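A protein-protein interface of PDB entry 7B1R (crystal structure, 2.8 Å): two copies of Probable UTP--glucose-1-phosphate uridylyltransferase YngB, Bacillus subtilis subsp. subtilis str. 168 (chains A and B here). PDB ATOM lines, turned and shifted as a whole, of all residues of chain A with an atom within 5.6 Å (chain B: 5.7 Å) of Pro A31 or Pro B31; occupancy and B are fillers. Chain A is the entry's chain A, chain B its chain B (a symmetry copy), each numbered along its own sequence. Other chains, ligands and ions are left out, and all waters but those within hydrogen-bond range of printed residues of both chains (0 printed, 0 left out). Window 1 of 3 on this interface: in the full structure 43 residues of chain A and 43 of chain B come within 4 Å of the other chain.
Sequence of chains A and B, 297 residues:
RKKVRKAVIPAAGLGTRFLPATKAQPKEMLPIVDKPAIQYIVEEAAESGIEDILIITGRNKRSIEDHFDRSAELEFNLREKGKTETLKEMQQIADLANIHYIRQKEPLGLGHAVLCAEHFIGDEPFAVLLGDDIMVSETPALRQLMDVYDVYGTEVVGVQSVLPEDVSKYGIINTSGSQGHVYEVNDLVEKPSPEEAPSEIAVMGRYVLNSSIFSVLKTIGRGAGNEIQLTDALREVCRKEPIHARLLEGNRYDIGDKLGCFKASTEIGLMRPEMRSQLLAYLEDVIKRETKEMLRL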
ATOM      1  N   ALA A  21      10.075  -9.427  -2.285  1.00  0.00           N
ATOM      2  CA  ALA A  21      11.122  -9.355  -3.301  1.00  0.00           C
ATOM      3  C   ALA A  21      12.251  -8.478  -2.803  1.00  0.00           C
ATOM      4  O   ALA A  21      13.415  -8.868  -2.847  1.00  0.00           O
ATOM      5  CB  ALA A  21      10.574  -8.757  -4.574  1.00  0.00           C
ATOM      6  N   GLN A  25      17.076  -7.074  -0.971  1.00  0.00           N
ATOM      7  CA  GLN A  25      17.717  -6.566  -2.164  1.00  0.00           C
ATOM      8  C   GLN A  25      16.954  -5.338  -2.657  1.00  0.00           C
ATOM      9  O   GLN A  25      15.746  -5.238  -2.465  1.00  0.00           O
ATOM     10  CB  GLN A  25      17.822  -7.698  -3.177  1.00  0.00           C
ATOM     11  CG  GLN A  25      16.477  -8.147  -3.693  1.00  0.00           C
ATOM     12  CD  GLN A  25      16.677  -9.223  -4.732  1.00  0.00           C
ATOM     13  OE1 GLN A  25      17.815  -9.677  -4.958  1.00  0.00           O
ATOM     14  NE2 GLN A  25      15.569  -9.625  -5.360  1.00  0.00           N
ATOM     15  N   MET A  29      17.016  -2.595  -8.277  1.00  0.00           N
ATOM     16  CA  MET A  29      17.670  -3.692  -8.970  1.00  0.00           C
ATOM     17  C   MET A  29      16.657  -4.687  -9.523  1.00  0.00           C
ATOM     18  O   MET A  29      17.048  -5.595 -10.243  1.00  0.00           O
ATOM     19  CB  MET A  29      18.689  -4.402  -8.072  1.00  0.00           C
ATOM     20  CG  MET A  29      19.934  -3.599  -7.762  1.00  0.00           C
ATOM     21  SD  MET A  29      20.882  -3.214  -9.437  1.00  0.00           S
ATOM     22  CE  MET A  29      21.864  -4.874  -9.811  1.00  0.00           C
ATOM     23  N   LEU A  30      15.370  -4.522  -9.218  1.00  0.00           N
ATOM     24  CA  LEU A  30      14.385  -5.469  -9.729  1.00  0.00           C
ATOM     25  C   LEU A  30      14.373  -5.392 -11.244  1.00  0.00           C
ATOM     26  O   LEU A  30      14.413  -4.311 -11.832  1.00  0.00           O
ATOM     27  CB  LEU A  30      12.988  -5.161  -9.193  1.00  0.00           C
ATOM     28  CG  LEU A  30      12.810  -5.332  -7.681  1.00  0.00           C
ATOM     29  CD1 LEU A  30      11.594  -4.570  -7.176  1.00  0.00           C
ATOM     30  CD2 LEU A  30      12.678  -6.798  -7.326  1.00  0.00           C
ATOM     31  N   PRO A  31      14.322  -6.551 -11.922  1.00  0.00           N
ATOM     32  CA  PRO A  31      14.452  -6.572 -13.379  1.00  0.00           C
ATOM     33  C   PRO A  31      13.175  -6.027 -14.010  1.00  0.00           C
ATOM     34  O   PRO A  31      12.093  -6.246 -13.493  1.00  0.00           O
ATOM     35  CB  PRO A  31      14.694  -8.057 -13.677  1.00  0.00           C
ATOM     36  CG  PRO A  31      14.017  -8.795 -12.523  1.00  0.00           C
ATOM     37  CD  PRO A  31      14.102  -7.875 -11.324  1.00  0.00           C
ATOM     38  N   ILE A  32      13.311  -5.260 -15.089  1.00  0.00           N
ATOM     39  CA  ILE A  32      12.136  -4.961 -15.866  1.00  0.00           C
ATOM     40  C   ILE A  32      12.072  -5.992 -16.972  1.00  0.00           C
ATOM     41  O   ILE A  32      11.326  -6.962 -16.830  1.00  0.00           O
ATOM     42  CB  ILE A  32      12.062  -3.508 -16.337  1.00  0.00           C
ATOM     43  CG1 ILE A  32      11.792  -2.612 -15.126  1.00  0.00           C
ATOM     44  CG2 ILE A  32      10.973  -3.363 -17.392  1.00  0.00           C
ATOM     45  CD1 ILE A  32      10.739  -3.170 -14.211  1.00  0.00           C
ATOM     46  N   VAL A  33      12.864  -5.871 -18.038  1.00  0.00           N
ATOM     47  CA  VAL A  33      12.699  -7.057 -18.871  1.00  0.00           C
ATOM     48  C   VAL A  33      13.734  -8.105 -18.458  1.00  0.00           C
ATOM     49  O   VAL A  33      13.421  -9.181 -17.961  1.00  0.00           O
ATOM     50  CB  VAL A  33      12.624  -6.798 -20.384  1.00  0.00           C
ATOM     51  CG1 VAL A  33      12.754  -8.108 -21.135  1.00  0.00           C
ATOM     52  CG2 VAL A  33      11.310  -6.141 -20.757  1.00  0.00           C
ATOM     53  N   ASP A  34      14.985  -7.718 -18.579  1.00  0.00           N
ATOM     54  CA  ASP A  34      16.095  -8.563 -18.231  1.00  0.00           C
ATOM     55  C   ASP A  34      17.151  -7.619 -17.669  1.00  0.00           C
ATOM     56  O   ASP A  34      18.250  -8.038 -17.312  1.00  0.00           O
ATOM     57  CB  ASP A  34      16.574  -9.303 -19.487  1.00  0.00           C
ATOM     58  CG  ASP A  34      16.982  -8.415 -20.647  1.00  0.00           C
ATOM     59  OD1 ASP A  34      16.526  -7.252 -20.711  1.00  0.00           O
ATOM     60  OD2 ASP A  34      17.747  -8.911 -21.483  1.00  0.00           O
ATOM     61  N   LYS A  35      16.815  -6.325 -17.633  1.00  0.00           N
ATOM     62  CA  LYS A  35      17.714  -5.305 -17.134  1.00  0.00           C
ATOM     63  C   LYS A  35      17.166  -4.718 -15.835  1.00  0.00           C
ATOM     64  O   LYS A  35      15.965  -4.499 -15.691  1.00  0.00           O
ATOM     65  CB  LYS A  35      17.825  -4.161 -18.137  1.00  0.00           C
ATOM     66  CG  LYS A  35      17.943  -4.605 -19.580  1.00  0.00           C
ATOM     67  CD  LYS A  35      18.650  -3.581 -20.426  1.00  0.00           C
ATOM     68  CE  LYS A  35      18.015  -2.224 -20.276  1.00  0.00           C
ATOM     69  NZ  LYS A  35      18.154  -1.484 -21.544  1.00  0.00           N
ATOM     70  N   PRO A  36      18.024  -4.461 -14.827  1.00  0.00           N
ATOM     71  CA  PRO A  36      17.596  -3.737 -13.634  1.00  0.00           C
ATOM     72  C   PRO A  36      16.977  -2.380 -13.939  1.00  0.00           C
ATOM     73  O   PRO A  36      17.389  -1.670 -14.858  1.00  0.00           O
ATOM     74  CB  PRO A  36      18.897  -3.617 -12.844  1.00  0.00           C
ATOM     75  CG  PRO A  36      19.581  -4.903 -13.201  1.00  0.00           C
ATOM     76  CD  PRO A  36      19.392  -4.981 -14.704  1.00  0.00           C
ATOM     77  N   ALA A  37      15.957  -2.060 -13.142  1.00  0.00           N
ATOM     78  CA  ALA A  37      15.201  -0.846 -13.340  1.00  0.00           C
ATOM     79  C   ALA A  37      16.182   0.321 -13.384  1.00  0.00           C
ATOM     80  O   ALA A  37      16.106   1.219 -14.232  1.00  0.00           O
ATOM     81  CB  ALA A  37      14.225  -0.709 -12.214  1.00  0.00           C
ATOM     82  N   SER A 265       7.224  -4.917 -18.220  1.00  0.00           N
ATOM     83  CA  SER A 265       7.970  -6.045 -18.750  1.00  0.00           C
ATOM     84  C   SER A 265       7.348  -6.548 -20.058  1.00  0.00           C
ATOM     85  O   SER A 265       8.044  -6.914 -20.994  1.00  0.00           O
ATOM     86  CB  SER A 265       8.034  -7.141 -17.743  1.00  0.00           C
ATOM     87  OG  SER A 265       8.777  -6.734 -16.630  1.00  0.00           O
ATOM     88  N   ALA B  21      20.349  -9.099 -15.737  1.00  0.00           N
ATOM     89  CA  ALA B  21      19.676  -8.999 -14.454  1.00  0.00           C
ATOM     90  C   ALA B  21      20.611  -9.524 -13.367  1.00  0.00           C
ATOM     91  O   ALA B  21      20.562  -9.061 -12.224  1.00  0.00           O
ATOM     92  CB  ALA B  21      18.395  -9.781 -14.466  1.00  0.00           C
ATOM     93  N   GLN B  25      23.736  -9.595  -9.021  1.00  0.00           N
ATOM     94  CA  GLN B  25      22.857 -10.205  -8.037  1.00  0.00           C
ATOM     95  C   GLN B  25      22.457 -11.615  -8.470  1.00  0.00           C
ATOM     96  O   GLN B  25      22.442 -11.948  -9.646  1.00  0.00           O
ATOM     97  CB  GLN B  25      21.673  -9.287  -7.762  1.00  0.00           C
ATOM     98  CG  GLN B  25      20.750  -9.077  -8.947  1.00  0.00           C
ATOM     99  CD  GLN B  25      19.821  -7.913  -8.695  1.00  0.00           C
ATOM    100  OE1 GLN B  25      19.830  -7.297  -7.623  1.00  0.00           O
ATOM    101  NE2 GLN B  25      19.028  -7.583  -9.706  1.00  0.00           N
ATOM    102  N   MET B  29      17.339 -15.109  -6.602  1.00  0.00           N
ATOM    103  CA  MET B  29      16.683 -13.982  -5.956  1.00  0.00           C
ATOM    104  C   MET B  29      15.796 -13.237  -6.941  1.00  0.00           C
ATOM    105  O   MET B  29      14.956 -12.444  -6.529  1.00  0.00           O
ATOM    106  CB  MET B  29      17.696 -13.012  -5.348  1.00  0.00           C
ATOM    107  CG  MET B  29      18.466 -13.572  -4.182  1.00  0.00           C
ATOM    108  SD  MET B  29      17.287 -13.935  -2.661  1.00  0.00           S
ATOM    109  CE  MET B  29      16.905 -12.152  -1.917  1.00  0.00           C
ATOM    110  N   LEU B  30      15.988 -13.467  -8.243  1.00  0.00           N
ATOM    111  CA  LEU B  30      15.048 -12.910  -9.204  1.00  0.00           C
ATOM    112  C   LEU B  30      13.625 -13.206  -8.732  1.00  0.00           C
ATOM    113  O   LEU B  30      13.242 -14.328  -8.361  1.00  0.00           O
ATOM    114  CB  LEU B  30      15.288 -13.476 -10.606  1.00  0.00           C
ATOM    115  CG  LEU B  30      16.657 -13.215 -11.233  1.00  0.00           C
ATOM    116  CD1 LEU B  30      16.743 -14.034 -12.504  1.00  0.00           C
ATOM    117  CD2 LEU B  30      16.888 -11.731 -11.553  1.00  0.00           C
ATOM    118  N   PRO B  31      12.800 -12.152  -8.692  1.00  0.00           N
ATOM    119  CA  PRO B  31      11.440 -12.280  -8.177  1.00  0.00           C
ATOM    120  C   PRO B  31      10.594 -13.122  -9.125  1.00  0.00           C
ATOM    121  O   PRO B  31      10.760 -13.010 -10.342  1.00  0.00           O
ATOM    122  CB  PRO B  31      10.975 -10.816  -8.160  1.00  0.00           C
ATOM    123  CG  PRO B  31      11.807 -10.133  -9.230  1.00  0.00           C
ATOM    124  CD  PRO B  31      13.160 -10.803  -9.155  1.00  0.00           C
ATOM    125  N   ILE B  32       9.691 -13.942  -8.555  1.00  0.00           N
ATOM    126  CA  ILE B  32       8.800 -14.755  -9.370  1.00  0.00           C
ATOM    127  C   ILE B  32       7.402 -14.161  -9.417  1.00  0.00           C
ATOM    128  O   ILE B  32       6.908 -13.810 -10.487  1.00  0.00           O
ATOM    129  CB  ILE B  32       8.833 -16.255  -9.054  1.00  0.00           C
ATOM    130  CG1 ILE B  32       9.937 -16.928  -9.875  1.00  0.00           C
ATOM    131  CG2 ILE B  32       7.477 -16.897  -9.295  1.00  0.00           C
ATOM    132  CD1 ILE B  32      10.080 -16.361 -11.240  1.00  0.00           C
ATOM    133  N   VAL B  33       6.745 -13.957  -8.291  1.00  0.00           N
ATOM    134  CA  VAL B  33       5.732 -12.943  -8.562  1.00  0.00           C
ATOM    135  C   VAL B  33       6.200 -11.641  -7.922  1.00  0.00           C
ATOM    136  O   VAL B  33       6.543 -10.672  -8.584  1.00  0.00           O
ATOM    137  CB  VAL B  33       4.316 -13.384  -8.170  1.00  0.00           C
ATOM    138  CG1 VAL B  33       3.418 -12.199  -7.937  1.00  0.00           C
ATOM    139  CG2 VAL B  33       3.736 -14.314  -9.226  1.00  0.00           C
ATOM    140  N   ASP B  34       6.332 -11.700  -6.614  1.00  0.00           N
ATOM    141  CA  ASP B  34       7.021 -10.686  -5.857  1.00  0.00           C
ATOM    142  C   ASP B  34       7.896 -11.427  -4.859  1.00  0.00           C
ATOM    143  O   ASP B  34       8.319 -10.840  -3.873  1.00  0.00           O
ATOM    144  CB  ASP B  34       5.996  -9.835  -5.113  1.00  0.00           C
ATOM    145  CG  ASP B  34       4.879 -10.646  -4.466  1.00  0.00           C
ATOM    146  OD1 ASP B  34       5.026 -11.902  -4.319  1.00  0.00           O
ATOM    147  OD2 ASP B  34       3.863 -10.020  -4.112  1.00  0.00           O
ATOM    148  N   LYS B  35       8.066 -12.739  -5.097  1.00  0.00           N
ATOM    149  CA  LYS B  35       8.868 -13.619  -4.262  1.00  0.00           C
ATOM    150  C   LYS B  35      10.132 -14.029  -5.013  1.00  0.00           C
ATOM    151  O   LYS B  35      10.092 -14.414  -6.183  1.00  0.00           O
ATOM    152  CB  LYS B  35       8.090 -14.892  -3.928  1.00  0.00           C
ATOM    153  CG  LYS B  35       7.156 -14.783  -2.744  1.00  0.00           C
ATOM    154  CD  LYS B  35       7.078 -16.089  -2.000  1.00  0.00           C
ATOM    155  CE  LYS B  35       6.107 -17.072  -2.615  1.00  0.00           C
ATOM    156  NZ  LYS B  35       5.098 -17.518  -1.619  1.00  0.00           N
ATOM    157  N   PRO B  36      11.299 -13.990  -4.348  1.00  0.00           N
ATOM    158  CA  PRO B  36      12.532 -14.559  -4.893  1.00  0.00           C
ATOM    159  C   PRO B  36      12.359 -16.047  -5.151  1.00  0.00           C
ATOM    160  O   PRO B  36      11.757 -16.755  -4.326  1.00  0.00           O
ATOM    161  CB  PRO B  36      13.489 -14.482  -3.716  1.00  0.00           C
ATOM    162  CG  PRO B  36      12.996 -13.314  -2.967  1.00  0.00           C
ATOM    163  CD  PRO B  36      11.486 -13.425  -3.013  1.00  0.00           C
ATOM    164  N   ALA B  37      12.891 -16.483  -6.304  1.00  0.00           N
ATOM    165  CA  ALA B  37      12.719 -17.860  -6.719  1.00  0.00           C
ATOM    166  C   ALA B  37      13.042 -18.775  -5.534  1.00  0.00           C
ATOM    167  O   ALA B  37      12.240 -19.648  -5.181  1.00  0.00           O
ATOM    168  CB  ALA B  37      13.559 -18.173  -7.941  1.00  0.00           C
ATOM    169  N   SER B 265       5.585 -16.259 -13.677  1.00  0.00           N
ATOM    170  CA  SER B 265       5.099 -15.084 -12.978  1.00  0.00           C
ATOM    171  C   SER B 265       3.630 -14.842 -13.298  1.00  0.00           C
ATOM    172  O   SER B 265       2.842 -14.499 -12.414  1.00  0.00           O
ATOM    173  CB  SER B 265       5.903 -13.889 -13.350  1.00  0.00           C
ATOM    174  OG  SER B 265       7.238 -14.082 -12.945  1.00  0.00           O
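Among the printed residues, pairs that only touch across the chains: Leu A30 with Pro B31 (3.9 Å) and Pro A31 with Pro B31 (3.8 Å).
The side-chain amide nitrogen of Gln A25 lies close to the backbone carbonyl oxygen of Ala A21 (3.4 Å). The backbone carbonyl oxygen (O) of Leu A30 lies within hydrogen-bond range of the backbone NH (N) of Ala A37. NE2 of Gln B25 sits close to O of Ala B21, at 3.3 Å.
Ala A21 touches Asp B34, and with the chains exchanged Asp A34 touches Ala B21. Gln A25 touches Met B29, and with the chains exchanged Met A29 touches Gln B25. Leu A30 touches Pro B31, but with the chains exchanged Pro A31 does not touch Leu B30 (4.2 Å). Pro B31 touches its own counterpart, Pro A31. Positions printed for both chains: 21, 25, 29, 30, 31, 32, 33, 34, 35, 36, 37 and 265. Of the 6 pairs that touch across the chains among the printed residues, 5 have their exchanged pair printed and touching as well.
Of the 12 printed residues of chain B, 5 touch a printed residue of chain A. Printed residues of chain B that touch a printed residue of chain A: Ala B21, Gln B25, Met B29, Pro B31 and Asp B34. Along chain B the printed residues that touch a printed residue of chain A span positions 21 to 34. Of the 12 printed residues of chain A, 6 touch a printed residue of chain B. Printed residues of chain A that touch a printed residue of chain B: Ala A21, Gln A25, Met A29, Leu A30, Pro A31 and Asp A34. Hydrophobic or aromatic side chains of chain A that line the printed part of chain B: Ala A21, Met A29, Leu A30 and Pro A31. Among the printed residues, 6 pairs touch across the chains. Among the printed residues, no Asp or Glu carboxylate lies within 4 Å of a Lys or Arg side-chain nitrogen of the other chain.
Pro A31 touches one residue of chain B. Of the printed residues of chain B, Leu A30 touches Pro B31. Of the printed residues of chain B, Met A29 touches Gln B25 (2.9 Å). The nearest residue of chain B that does not touch Pro A31 is Ala B21 (4.2 Å). The nearest residue of chain A that does not touch Pro B31 is Ala A21 (4.2 Å).
The backbone NH of Ala A21 lies within hydrogen-bond range of the backbone carbonyl oxygen of Asp B34, at 2.8 Å. NE2 of Gln A25 lies within hydrogen-bond range of O of Met B29. O of Met A29 sits at hydrogen-bond distance from NE2 of Gln B25 (2.9 Å). N of Ala B21 is in hydrogen-bond range of O of Asp A34 (2.8 Å).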
